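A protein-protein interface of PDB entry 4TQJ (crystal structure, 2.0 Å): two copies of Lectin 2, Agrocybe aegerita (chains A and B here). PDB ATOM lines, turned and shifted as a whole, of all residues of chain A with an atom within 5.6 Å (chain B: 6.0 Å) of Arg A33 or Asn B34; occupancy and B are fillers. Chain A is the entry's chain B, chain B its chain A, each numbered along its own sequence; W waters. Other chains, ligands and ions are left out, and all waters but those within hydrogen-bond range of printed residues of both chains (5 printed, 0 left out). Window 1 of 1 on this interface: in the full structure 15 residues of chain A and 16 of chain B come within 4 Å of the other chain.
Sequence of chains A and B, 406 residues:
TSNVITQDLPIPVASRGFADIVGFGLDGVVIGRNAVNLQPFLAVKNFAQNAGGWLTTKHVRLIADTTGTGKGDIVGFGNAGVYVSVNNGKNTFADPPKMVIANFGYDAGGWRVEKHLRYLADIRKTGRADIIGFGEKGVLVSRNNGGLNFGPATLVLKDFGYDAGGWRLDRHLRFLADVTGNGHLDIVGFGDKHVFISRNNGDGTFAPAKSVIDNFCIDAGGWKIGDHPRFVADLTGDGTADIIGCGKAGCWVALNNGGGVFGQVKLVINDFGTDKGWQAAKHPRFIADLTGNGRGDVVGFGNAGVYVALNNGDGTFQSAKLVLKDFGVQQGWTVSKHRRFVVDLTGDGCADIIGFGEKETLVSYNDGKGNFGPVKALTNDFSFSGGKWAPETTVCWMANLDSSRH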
ATOM      1  N   ASP A  20     -22.464  12.920  19.927  1.00  0.00           N
ATOM      2  CA  ASP A  20     -21.574  13.987  20.367  1.00  0.00           C
ATOM      3  C   ASP A  20     -20.678  14.440  19.226  1.00  0.00           C
ATOM      4  O   ASP A  20     -20.346  13.657  18.330  1.00  0.00           O
ATOM      5  CB  ASP A  20     -20.701  13.502  21.515  1.00  0.00           C
ATOM      6  CG  ASP A  20     -21.508  12.964  22.675  1.00  0.00           C
ATOM      7  OD1 ASP A  20     -22.256  13.748  23.305  1.00  0.00           O
ATOM      8  OD2 ASP A  20     -21.373  11.755  22.968  1.00  0.00           O
ATOM      9  N   ILE A  21     -20.298  15.711  19.260  1.00  0.00           N
ATOM     10  CA  ILE A  21     -19.324  16.247  18.318  1.00  0.00           C
ATOM     11  C   ILE A  21     -17.935  15.946  18.839  1.00  0.00           C
ATOM     12  O   ILE A  21     -17.637  16.196  20.002  1.00  0.00           O
ATOM     13  CB  ILE A  21     -19.461  17.771  18.155  1.00  0.00           C
ATOM     14  CG1 ILE A  21     -20.840  18.128  17.602  1.00  0.00           C
ATOM     15  CG2 ILE A  21     -18.364  18.314  17.218  1.00  0.00           C
ATOM     16  CD1 ILE A  21     -21.162  19.612  17.692  1.00  0.00           C
ATOM     17  N   ILE A  31     -14.068  18.361  22.327  1.00  0.00           N
ATOM     18  CA  ILE A  31     -15.294  17.602  22.527  1.00  0.00           C
ATOM     19  C   ILE A  31     -16.477  18.559  22.589  1.00  0.00           C
ATOM     20  O   ILE A  31     -16.484  19.511  23.376  1.00  0.00           O
ATOM     21  CB  ILE A  31     -15.254  16.807  23.846  1.00  0.00           C
ATOM     22  CG1 ILE A  31     -13.967  15.978  23.949  1.00  0.00           C
ATOM     23  CG2 ILE A  31     -16.495  15.907  23.977  1.00  0.00           C
ATOM     24  CD1 ILE A  31     -13.933  14.797  23.008  1.00  0.00           C
ATOM     25  N   GLY A  32     -17.467  18.307  21.748  1.00  0.00           N
ATOM     26  CA  GLY A  32     -18.686  19.087  21.720  1.00  0.00           C
ATOM     27  C   GLY A  32     -19.780  18.178  22.218  1.00  0.00           C
ATOM     28  O   GLY A  32     -20.627  17.689  21.462  1.00  0.00           O
ATOM     29  N   ARG A  33     -19.752  17.916  23.512  1.00  0.00           N
ATOM     30  CA  ARG A  33     -20.611  16.878  24.030  1.00  0.00           C
ATOM     31  C   ARG A  33     -22.096  17.312  23.983  1.00  0.00           C
ATOM     32  O   ARG A  33     -22.441  18.465  24.274  1.00  0.00           O
ATOM     33  CB  ARG A  33     -20.087  16.419  25.387  1.00  0.00           C
ATOM     34  CG  ARG A  33     -21.109  16.180  26.414  1.00  0.00           C
ATOM     35  CD  ARG A  33     -21.629  14.782  26.433  1.00  0.00           C
ATOM     36  NE  ARG A  33     -23.009  14.916  26.845  1.00  0.00           N
ATOM     37  CZ  ARG A  33     -23.671  14.138  27.682  1.00  0.00           C
ATOM     38  NH1 ARG A  33     -23.116  13.067  28.218  1.00  0.00           N
ATOM     39  NH2 ARG A  33     -24.919  14.458  27.957  1.00  0.00           N
ATOM     40  N   ASN A  34     -22.944  16.407  23.507  1.00  0.00           N
ATOM     41  CA  ASN A  34     -24.357  16.689  23.291  1.00  0.00           C
ATOM     42  C   ASN A  34     -25.001  16.948  24.652  1.00  0.00           C
ATOM     43  O   ASN A  34     -25.200  16.010  25.428  1.00  0.00           O
ATOM     44  CB  ASN A  34     -25.002  15.486  22.613  1.00  0.00           C
ATOM     45  CG  ASN A  34     -26.463  15.714  22.251  1.00  0.00           C
ATOM     46  OD1 ASN A  34     -27.203  16.380  22.976  1.00  0.00           O
ATOM     47  ND2 ASN A  34     -26.888  15.139  21.123  1.00  0.00           N
ATOM     48  N   ALA A  35     -25.322  18.212  24.933  1.00  0.00           N
ATOM     49  CA  ALA A  35     -25.705  18.637  26.289  1.00  0.00           C
ATOM     50  C   ALA A  35     -26.415  19.981  26.260  1.00  0.00           C
ATOM     51  O   ALA A  35     -26.433  20.640  25.234  1.00  0.00           O
ATOM     52  CB  ALA A  35     -24.462  18.727  27.172  1.00  0.00           C
ATOM     53  N   VAL A  36     -26.981  20.397  27.394  1.00  0.00           N
ATOM     54  CA  VAL A  36     -27.822  21.597  27.439  1.00  0.00           C
ATOM     55  C   VAL A  36     -27.041  22.885  27.165  1.00  0.00           C
ATOM     56  O   VAL A  36     -27.588  23.848  26.632  1.00  0.00           O
ATOM     57  CB  VAL A  36     -28.582  21.725  28.789  1.00  0.00           C
ATOM     58  CG1 VAL A  36     -29.551  20.567  28.964  1.00  0.00           C
ATOM     59  CG2 VAL A  36     -27.605  21.792  29.954  1.00  0.00           C
ATOM     60  N   ASN A  37     -25.763  22.898  27.525  1.00  0.00           N
ATOM     61  CA  ASN A  37     -24.902  24.043  27.250  1.00  0.00           C
ATOM     62  C   ASN A  37     -23.698  23.611  26.423  1.00  0.00           C
ATOM     63  O   ASN A  37     -22.585  23.526  26.924  1.00  0.00           O
ATOM     64  CB  ASN A  37     -24.442  24.711  28.547  1.00  0.00           C
ATOM     65  CG  ASN A  37     -23.749  26.042  28.301  1.00  0.00           C
ATOM     66  OD1 ASN A  37     -23.997  26.703  27.290  1.00  0.00           O
ATOM     67  ND2 ASN A  37     -22.864  26.437  29.219  1.00  0.00           N
ATOM     68  N   LEU A  38     -23.937  23.330  25.150  1.00  0.00           N
ATOM     69  CA  LEU A  38     -22.890  22.825  24.271  1.00  0.00           C
ATOM     70  C   LEU A  38     -21.742  23.824  24.198  1.00  0.00           C
ATOM     71  O   LEU A  38     -21.930  24.968  23.805  1.00  0.00           O
ATOM     72  CB  LEU A  38     -23.459  22.535  22.874  1.00  0.00           C
ATOM     73  CG  LEU A  38     -22.570  21.870  21.815  1.00  0.00           C
ATOM     74  CD1 LEU A  38     -21.276  22.627  21.608  1.00  0.00           C
ATOM     75  CD2 LEU A  38     -22.285  20.421  22.151  1.00  0.00           C
ATOM     76  N   GLN A  39     -20.555  23.386  24.590  1.00  0.00           N
ATOM     77  CA  GLN A  39     -19.373  24.238  24.511  1.00  0.00           C
ATOM     78  C   GLN A  39     -18.170  23.396  24.118  1.00  0.00           C
ATOM     79  O   GLN A  39     -18.054  22.240  24.531  1.00  0.00           O
ATOM     80  CB  GLN A  39     -19.099  24.935  25.856  1.00  0.00           C
ATOM     81  CG  GLN A  39     -20.176  25.932  26.316  1.00  0.00           C
ATOM     82  CD  GLN A  39     -20.329  27.116  25.387  1.00  0.00           C
ATOM     83  OE1 GLN A  39     -19.415  27.459  24.640  1.00  0.00           O
ATOM     84  NE2 GLN A  39     -21.490  27.757  25.434  1.00  0.00           N
ATOM     85  N   ASN A  91     -15.659  12.428  31.763  1.00  0.00           N
ATOM     86  CA  ASN A  91     -15.285  13.459  30.791  1.00  0.00           C
ATOM     87  C   ASN A  91     -13.826  13.922  30.852  1.00  0.00           C
ATOM     88  O   ASN A  91     -13.535  15.095  30.627  1.00  0.00           O
ATOM     89  CB  ASN A  91     -16.215  14.673  30.882  1.00  0.00           C
ATOM     90  CG  ASN A  91     -16.049  15.617  29.711  1.00  0.00           C
ATOM     91  OD1 ASN A  91     -15.862  15.185  28.565  1.00  0.00           O
ATOM     92  ND2 ASN A  91     -16.092  16.916  29.988  1.00  0.00           N
ATOM     93  N   LEU A 401     -19.987   9.144  22.702  1.00  0.00           N
ATOM     94  CA  LEU A 401     -18.859   8.957  23.604  1.00  0.00           C
ATOM     95  C   LEU A 401     -19.232   7.984  24.696  1.00  0.00           C
ATOM     96  O   LEU A 401     -18.376   7.268  25.214  1.00  0.00           O
ATOM     97  CB  LEU A 401     -18.374  10.291  24.175  1.00  0.00           C
ATOM     98  CG  LEU A 401     -17.647  11.133  23.119  1.00  0.00           C
ATOM     99  CD1 LEU A 401     -17.456  12.568  23.565  1.00  0.00           C
ATOM    100  CD2 LEU A 401     -16.314  10.487  22.772  1.00  0.00           C
ATOM    101  N   ASP A 402     -20.520   7.943  25.015  1.00  0.00           N
ATOM    102  CA  ASP A 402     -21.041   7.037  26.028  1.00  0.00           C
ATOM    103  C   ASP A 402     -21.959   6.005  25.400  1.00  0.00           C
ATOM    104  O   ASP A 402     -23.158   6.245  25.266  1.00  0.00           O
ATOM    105  CB  ASP A 402     -21.844   7.830  27.070  1.00  0.00           C
ATOM    106  CG  ASP A 402     -20.966   8.590  28.034  1.00  0.00           C
ATOM    107  OD1 ASP A 402     -20.721   8.065  29.135  1.00  0.00           O
ATOM    108  OD2 ASP A 402     -20.526   9.703  27.690  1.00  0.00           O
ATOM    109  N   GLY B  17     -19.633  15.555  35.251  1.00  0.00           N
ATOM    110  CA  GLY B  17     -20.505  14.912  34.291  1.00  0.00           C
ATOM    111  C   GLY B  17     -21.655  15.784  33.798  1.00  0.00           C
ATOM    112  O   GLY B  17     -21.689  17.005  33.996  1.00  0.00           O
ATOM    113  N   PHE B  18     -22.616  15.149  33.141  1.00  0.00           N
ATOM    114  CA  PHE B  18     -23.737  15.881  32.585  1.00  0.00           C
ATOM    115  C   PHE B  18     -25.009  15.344  33.205  1.00  0.00           C
ATOM    116  O   PHE B  18     -25.653  14.449  32.653  1.00  0.00           O
ATOM    117  CB  PHE B  18     -23.757  15.752  31.065  1.00  0.00           C
ATOM    118  CG  PHE B  18     -22.438  16.072  30.416  1.00  0.00           C
ATOM    119  CD1 PHE B  18     -22.215  17.313  29.835  1.00  0.00           C
ATOM    120  CD2 PHE B  18     -21.420  15.140  30.394  1.00  0.00           C
ATOM    121  CE1 PHE B  18     -21.003  17.618  29.247  1.00  0.00           C
ATOM    122  CE2 PHE B  18     -20.202  15.438  29.802  1.00  0.00           C
ATOM    123  CZ  PHE B  18     -19.994  16.680  29.233  1.00  0.00           C
ATOM    124  N   ALA B  19     -25.368  15.867  34.377  1.00  0.00           N
ATOM    125  CA  ALA B  19     -26.535  15.326  35.068  1.00  0.00           C
ATOM    126  C   ALA B  19     -27.809  15.396  34.225  1.00  0.00           C
ATOM    127  O   ALA B  19     -28.080  16.400  33.564  1.00  0.00           O
ATOM    128  CB  ALA B  19     -26.748  16.015  36.444  1.00  0.00           C
ATOM    129  N   ASP B  20     -28.597  14.322  34.266  1.00  0.00           N
ATOM    130  CA  ASP B  20     -29.915  14.299  33.635  1.00  0.00           C
ATOM    131  C   ASP B  20     -31.035  14.549  34.648  1.00  0.00           C
ATOM    132  O   ASP B  20     -30.848  14.362  35.840  1.00  0.00           O
ATOM    133  CB  ASP B  20     -30.157  12.929  32.972  1.00  0.00           C
ATOM    134  CG  ASP B  20     -29.033  12.521  32.048  1.00  0.00           C
ATOM    135  OD1 ASP B  20     -28.872  13.155  30.991  1.00  0.00           O
ATOM    136  OD2 ASP B  20     -28.298  11.566  32.388  1.00  0.00           O
ATOM    137  N   ILE B  21     -32.206  14.959  34.170  1.00  0.00           N
ATOM    138  CA  ILE B  21     -33.369  15.141  35.041  1.00  0.00           C
ATOM    139  C   ILE B  21     -34.213  13.890  34.978  1.00  0.00           C
ATOM    140  O   ILE B  21     -34.522  13.409  33.893  1.00  0.00           O
ATOM    141  CB  ILE B  21     -34.271  16.282  34.569  1.00  0.00           C
ATOM    142  CG1 ILE B  21     -33.492  17.597  34.512  1.00  0.00           C
ATOM    143  CG2 ILE B  21     -35.495  16.423  35.490  1.00  0.00           C
ATOM    144  CD1 ILE B  21     -34.262  18.695  33.843  1.00  0.00           C
ATOM    145  N   GLY B  32     -35.653  13.912  31.353  1.00  0.00           N
ATOM    146  CA  GLY B  32     -35.085  15.083  30.713  1.00  0.00           C
ATOM    147  C   GLY B  32     -33.597  14.874  30.487  1.00  0.00           C
ATOM    148  O   GLY B  32     -32.763  15.376  31.249  1.00  0.00           O
ATOM    149  N   ARG B  33     -33.252  14.139  29.432  1.00  0.00           N
ATOM    150  CA  ARG B  33     -31.842  13.861  29.149  1.00  0.00           C
ATOM    151  C   ARG B  33     -31.045  15.134  28.823  1.00  0.00           C
ATOM    152  O   ARG B  33     -31.371  15.866  27.885  1.00  0.00           O
ATOM    153  CB  ARG B  33     -31.712  12.838  28.019  1.00  0.00           C
ATOM    154  CG  ARG B  33     -30.431  12.000  28.069  1.00  0.00           C
ATOM    155  CD  ARG B  33     -29.246  12.704  27.410  1.00  0.00           C
ATOM    156  NE  ARG B  33     -28.154  11.769  27.130  1.00  0.00           N
ATOM    157  CZ  ARG B  33     -27.037  12.096  26.489  1.00  0.00           C
ATOM    158  NH1 ARG B  33     -26.847  13.344  26.072  1.00  0.00           N
ATOM    159  NH2 ARG B  33     -26.100  11.179  26.272  1.00  0.00           N
ATOM    160  N   ASN B  34     -29.996  15.380  29.600  1.00  0.00           N
ATOM    161  CA  ASN B  34     -29.089  16.507  29.372  1.00  0.00           C
ATOM    162  C   ASN B  34     -28.558  16.455  27.931  1.00  0.00           C
ATOM    163  O   ASN B  34     -27.698  15.631  27.614  1.00  0.00           O
ATOM    164  CB  ASN B  34     -27.943  16.425  30.389  1.00  0.00           C
ATOM    165  CG  ASN B  34     -27.074  17.663  30.418  1.00  0.00           C
ATOM    166  OD1 ASN B  34     -26.826  18.286  29.393  1.00  0.00           O
ATOM    167  ND2 ASN B  34     -26.571  18.008  31.611  1.00  0.00           N
ATOM    168  N   ALA B  35     -29.070  17.326  27.060  1.00  0.00           N
ATOM    169  CA  ALA B  35     -28.786  17.231  25.621  1.00  0.00           C
ATOM    170  C   ALA B  35     -29.075  18.559  24.939  1.00  0.00           C
ATOM    171  O   ALA B  35     -29.649  19.451  25.549  1.00  0.00           O
ATOM    172  CB  ALA B  35     -29.625  16.115  24.977  1.00  0.00           C
ATOM    173  N   VAL B  36     -28.692  18.681  23.673  1.00  0.00           N
ATOM    174  CA  VAL B  36     -28.788  19.960  22.959  1.00  0.00           C
ATOM    175  C   VAL B  36     -30.221  20.447  22.775  1.00  0.00           C
ATOM    176  O   VAL B  36     -30.470  21.642  22.659  1.00  0.00           O
ATOM    177  CB  VAL B  36     -28.111  19.888  21.573  1.00  0.00           C
ATOM    178  CG1 VAL B  36     -26.599  19.656  21.729  1.00  0.00           C
ATOM    179  CG2 VAL B  36     -28.759  18.792  20.717  1.00  0.00           C
ATOM    180  N   LEU B  38     -33.231  19.792  24.914  1.00  0.00           N
ATOM    181  CA  LEU B  38     -33.832  19.194  26.098  1.00  0.00           C
ATOM    182  C   LEU B  38     -35.333  19.107  25.908  1.00  0.00           C
ATOM    183  O   LEU B  38     -35.997  20.121  25.715  1.00  0.00           O
ATOM    184  CB  LEU B  38     -33.508  20.001  27.355  1.00  0.00           C
ATOM    185  CG  LEU B  38     -34.224  19.541  28.634  1.00  0.00           C
ATOM    186  CD1 LEU B  38     -33.793  18.131  29.017  1.00  0.00           C
ATOM    187  CD2 LEU B  38     -33.989  20.512  29.790  1.00  0.00           C
ATOM    188  N   ASP B 344     -23.111  19.197  38.465  1.00  0.00           N
ATOM    189  CA  ASP B 344     -22.423  19.487  37.217  1.00  0.00           C
ATOM    190  C   ASP B 344     -23.338  19.102  36.058  1.00  0.00           C
ATOM    191  O   ASP B 344     -23.778  17.953  35.949  1.00  0.00           O
ATOM    192  CB  ASP B 344     -21.101  18.712  37.140  1.00  0.00           C
ATOM    193  CG  ASP B 344     -20.200  19.187  36.017  1.00  0.00           C
ATOM    194  OD1 ASP B 344     -20.447  20.301  35.497  1.00  0.00           O
ATOM    195  OD2 ASP B 344     -19.241  18.443  35.658  1.00  0.00           O
ATOM    196  N   LEU B 345     -23.641  20.078  35.214  1.00  0.00           N
ATOM    197  CA  LEU B 345     -24.426  19.842  34.009  1.00  0.00           C
ATOM    198  C   LEU B 345     -23.549  19.860  32.761  1.00  0.00           C
ATOM    199  O   LEU B 345     -24.030  19.560  31.657  1.00  0.00           O
ATOM    200  CB  LEU B 345     -25.496  20.916  33.861  1.00  0.00           C
ATOM    201  CG  LEU B 345     -26.541  20.984  34.959  1.00  0.00           C
ATOM    202  CD1 LEU B 345     -27.375  22.279  34.825  1.00  0.00           C
ATOM    203  CD2 LEU B 345     -27.405  19.741  34.889  1.00  0.00           C
ATOM    204  N   THR B 346     -22.272  20.217  32.928  1.00  0.00           N
ATOM    205  CA  THR B 346     -21.443  20.580  31.773  1.00  0.00           C
ATOM    206  C   THR B 346     -20.101  19.858  31.641  1.00  0.00           C
ATOM    207  O   THR B 346     -19.300  20.210  30.781  1.00  0.00           O
ATOM    208  CB  THR B 346     -21.141  22.090  31.760  1.00  0.00           C
ATOM    209  OG1 THR B 346     -20.209  22.391  32.808  1.00  0.00           O
ATOM    210  CG2 THR B 346     -22.408  22.888  31.947  1.00  0.00           C
ATOM    211  N   ASP B 402     -26.307   7.738  32.245  1.00  0.00           N
ATOM    212  CA  ASP B 402     -25.144   7.014  31.753  1.00  0.00           C
ATOM    213  C   ASP B 402     -23.976   7.148  32.736  1.00  0.00           C
ATOM    214  O   ASP B 402     -23.170   8.070  32.636  1.00  0.00           O
ATOM    215  CB  ASP B 402     -24.757   7.544  30.371  1.00  0.00           C
ATOM    216  CG  ASP B 402     -25.733   7.111  29.284  1.00  0.00           C
ATOM    217  OD1 ASP B 402     -26.033   5.896  29.197  1.00  0.00           O
ATOM    218  OD2 ASP B 402     -26.205   7.984  28.517  1.00  0.00           O
HETATM  219  O   HOH W   1     -26.250  13.241  30.174  1.00  0.00           O
HETATM  220  O   HOH W   2     -23.862  21.371  29.229  1.00  0.00           O
HETATM  221  O   HOH W   3     -24.246  12.340  24.504  1.00  0.00           O
HETATM  222  O   HOH W   4     -17.405  19.858  28.874  1.00  0.00           O
HETATM  223  O   HOH W   5     -21.337  21.055  28.228  1.00  0.00           O
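Water W4 bridges O of Thr B346 (2.7 Å) and ND2 of Asn A91 (3.4 Å). Water W3 bridges the side-chain carboxylate of Asp A20 (2.7 Å) and the guanidinium group of Arg B33 (2.8 Å). Water W1 lies within hydrogen-bond range of OD1 of Asp B20 (2.7 Å), O of Phe B18 (2.8 Å) and NH2 of Arg A33 (2.9 Å). Water W2 lies within hydrogen-bond range of N of Asn A37 (3.0 Å) and O of Leu B345 (3.0 Å). Water W5 lies within hydrogen-bond range of O of Asn A37 (3.1 Å) and O of Thr B346 (3.4 Å).
Asn A34 touches its own counterpart, Asn B34. Asn A34 touches Ala B35, and with the chains exchanged Ala A35 touches Asn B34. Asn A34 touches Val B36, and with the chains exchanged Val A36 touches Asn B34. Ala B35 touches its own counterpart, Ala A35. Positions printed for both chains: 20, 21, 32, 33, 34, 35, 36, 38 and 402. Of the 14 pairs that touch across the chains among the printed residues, 11 have their exchanged pair printed and touching as well.
Among the printed residues, pairs that only touch across the chains: Arg A33 with Phe B18, Asn A34 with Ala B35, Ala A35 with Asn B34, Ala A35 with Phe B18 and Asn A91 with Phe B18.
The backbone carbonyl oxygen (O) of Ala B19 is in hydrogen-bond range of the side-chain amide nitrogen (ND2) of Asn B34 (2.9 Å). The backbone NH (N) of Asn B34 is in hydrogen-bond range of the side-chain carboxylate (OD1) of Asp B20, at 2.9 Å. The side-chain carboxylate (OD2) of Asp B402 lies within salt-bridge range of the guanidinium group (NH2) of Arg B33, at 3.9 Å. O of Leu B345 is in hydrogen-bond range of ND2 of Asn B34, 3.0 Å away. The side-chain carboxylate of Asp A20 is in salt-bridge range of the guanidinium group of Arg A33. N of Asn A34 is in hydrogen-bond range of OD1 of Asp A20, 2.8 Å away.
Arg A33 touches just these residues of chain B: Phe B18 (3.1 Å), Arg B33 (2.9 Å) and Asn B34 (3.0 Å). Of the printed residues of chain B, Asn A34 touches Arg B33, Asn B34, Ala B35 and Val B36. Of the printed residues of chain B, Ala A35 touches Phe B18, Asn B34, Ala B35 and Val B36. Printed residues of chain A within 4 Å of Phe B18: Arg A33 (3.1 Å), Ala A35 (3.8 Å) and Asn A91 (3.98 Å). Of the printed residues of chain A, Arg B33 touches Arg A33 and Asn A34. Of chain A, only Arg A33 (3.0 Å), Asn A34 (3.3 Å), Ala A35 (3.3 Å) and Val A36 (2.9 Å) come within 4 Å of Asn B34. Printed residues of chain A within 4 Å of Ala B35: Asn A34 (3.2 Å), Ala A35 (3.3 Å) and Val A36 (3.4 Å). The nearest residue of chain B that does not touch Arg A33 is Val B36 (5.0 Å).
The guanidinium group of Arg B33 sits at hydrogen-bond distance from the backbone carbonyl oxygen of Asn A34 (3.2 Å). The backbone carbonyl oxygen of Asn B34 sits at hydrogen-bond distance from the guanidinium group of Arg A33, at 3.0 Å. OD1 of Asn B34 lies within hydrogen-bond range of N of Val A36. The backbone carbonyl oxygen of Ala B35 lies within hydrogen-bond range of the backbone NH of Val A36 (3.4 Å). N of Val B36 lies within hydrogen-bond range of OD1 of Asn A34, at 2.8 Å. The backbone carbonyl oxygen of Ala A35 lies close to the backbone NH of Val B36 (3.4 Å). The guanidinium group (NH1) of Arg B33 lies close to the guanidinium group (NH2) of Arg A33. O of Asn A34 sits close to O of Asn B34, 3.3 Å away. O of Ala B35 sits close to O of Ala A35, at 3.4 Å.
Hydrophobic or aromatic side chains of chain B that line the printed part of chain A: Phe B18, Ala B35 and Val B36. Printed residues of chain A that touch a printed residue of chain B: Arg A33, Asn A34, Ala A35, Val A36 and Asn A91. Among the printed residues, no Asp or Glu carboxylate lies within 4 Å of a Lys or Arg side-chain nitrogen of the other chain.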
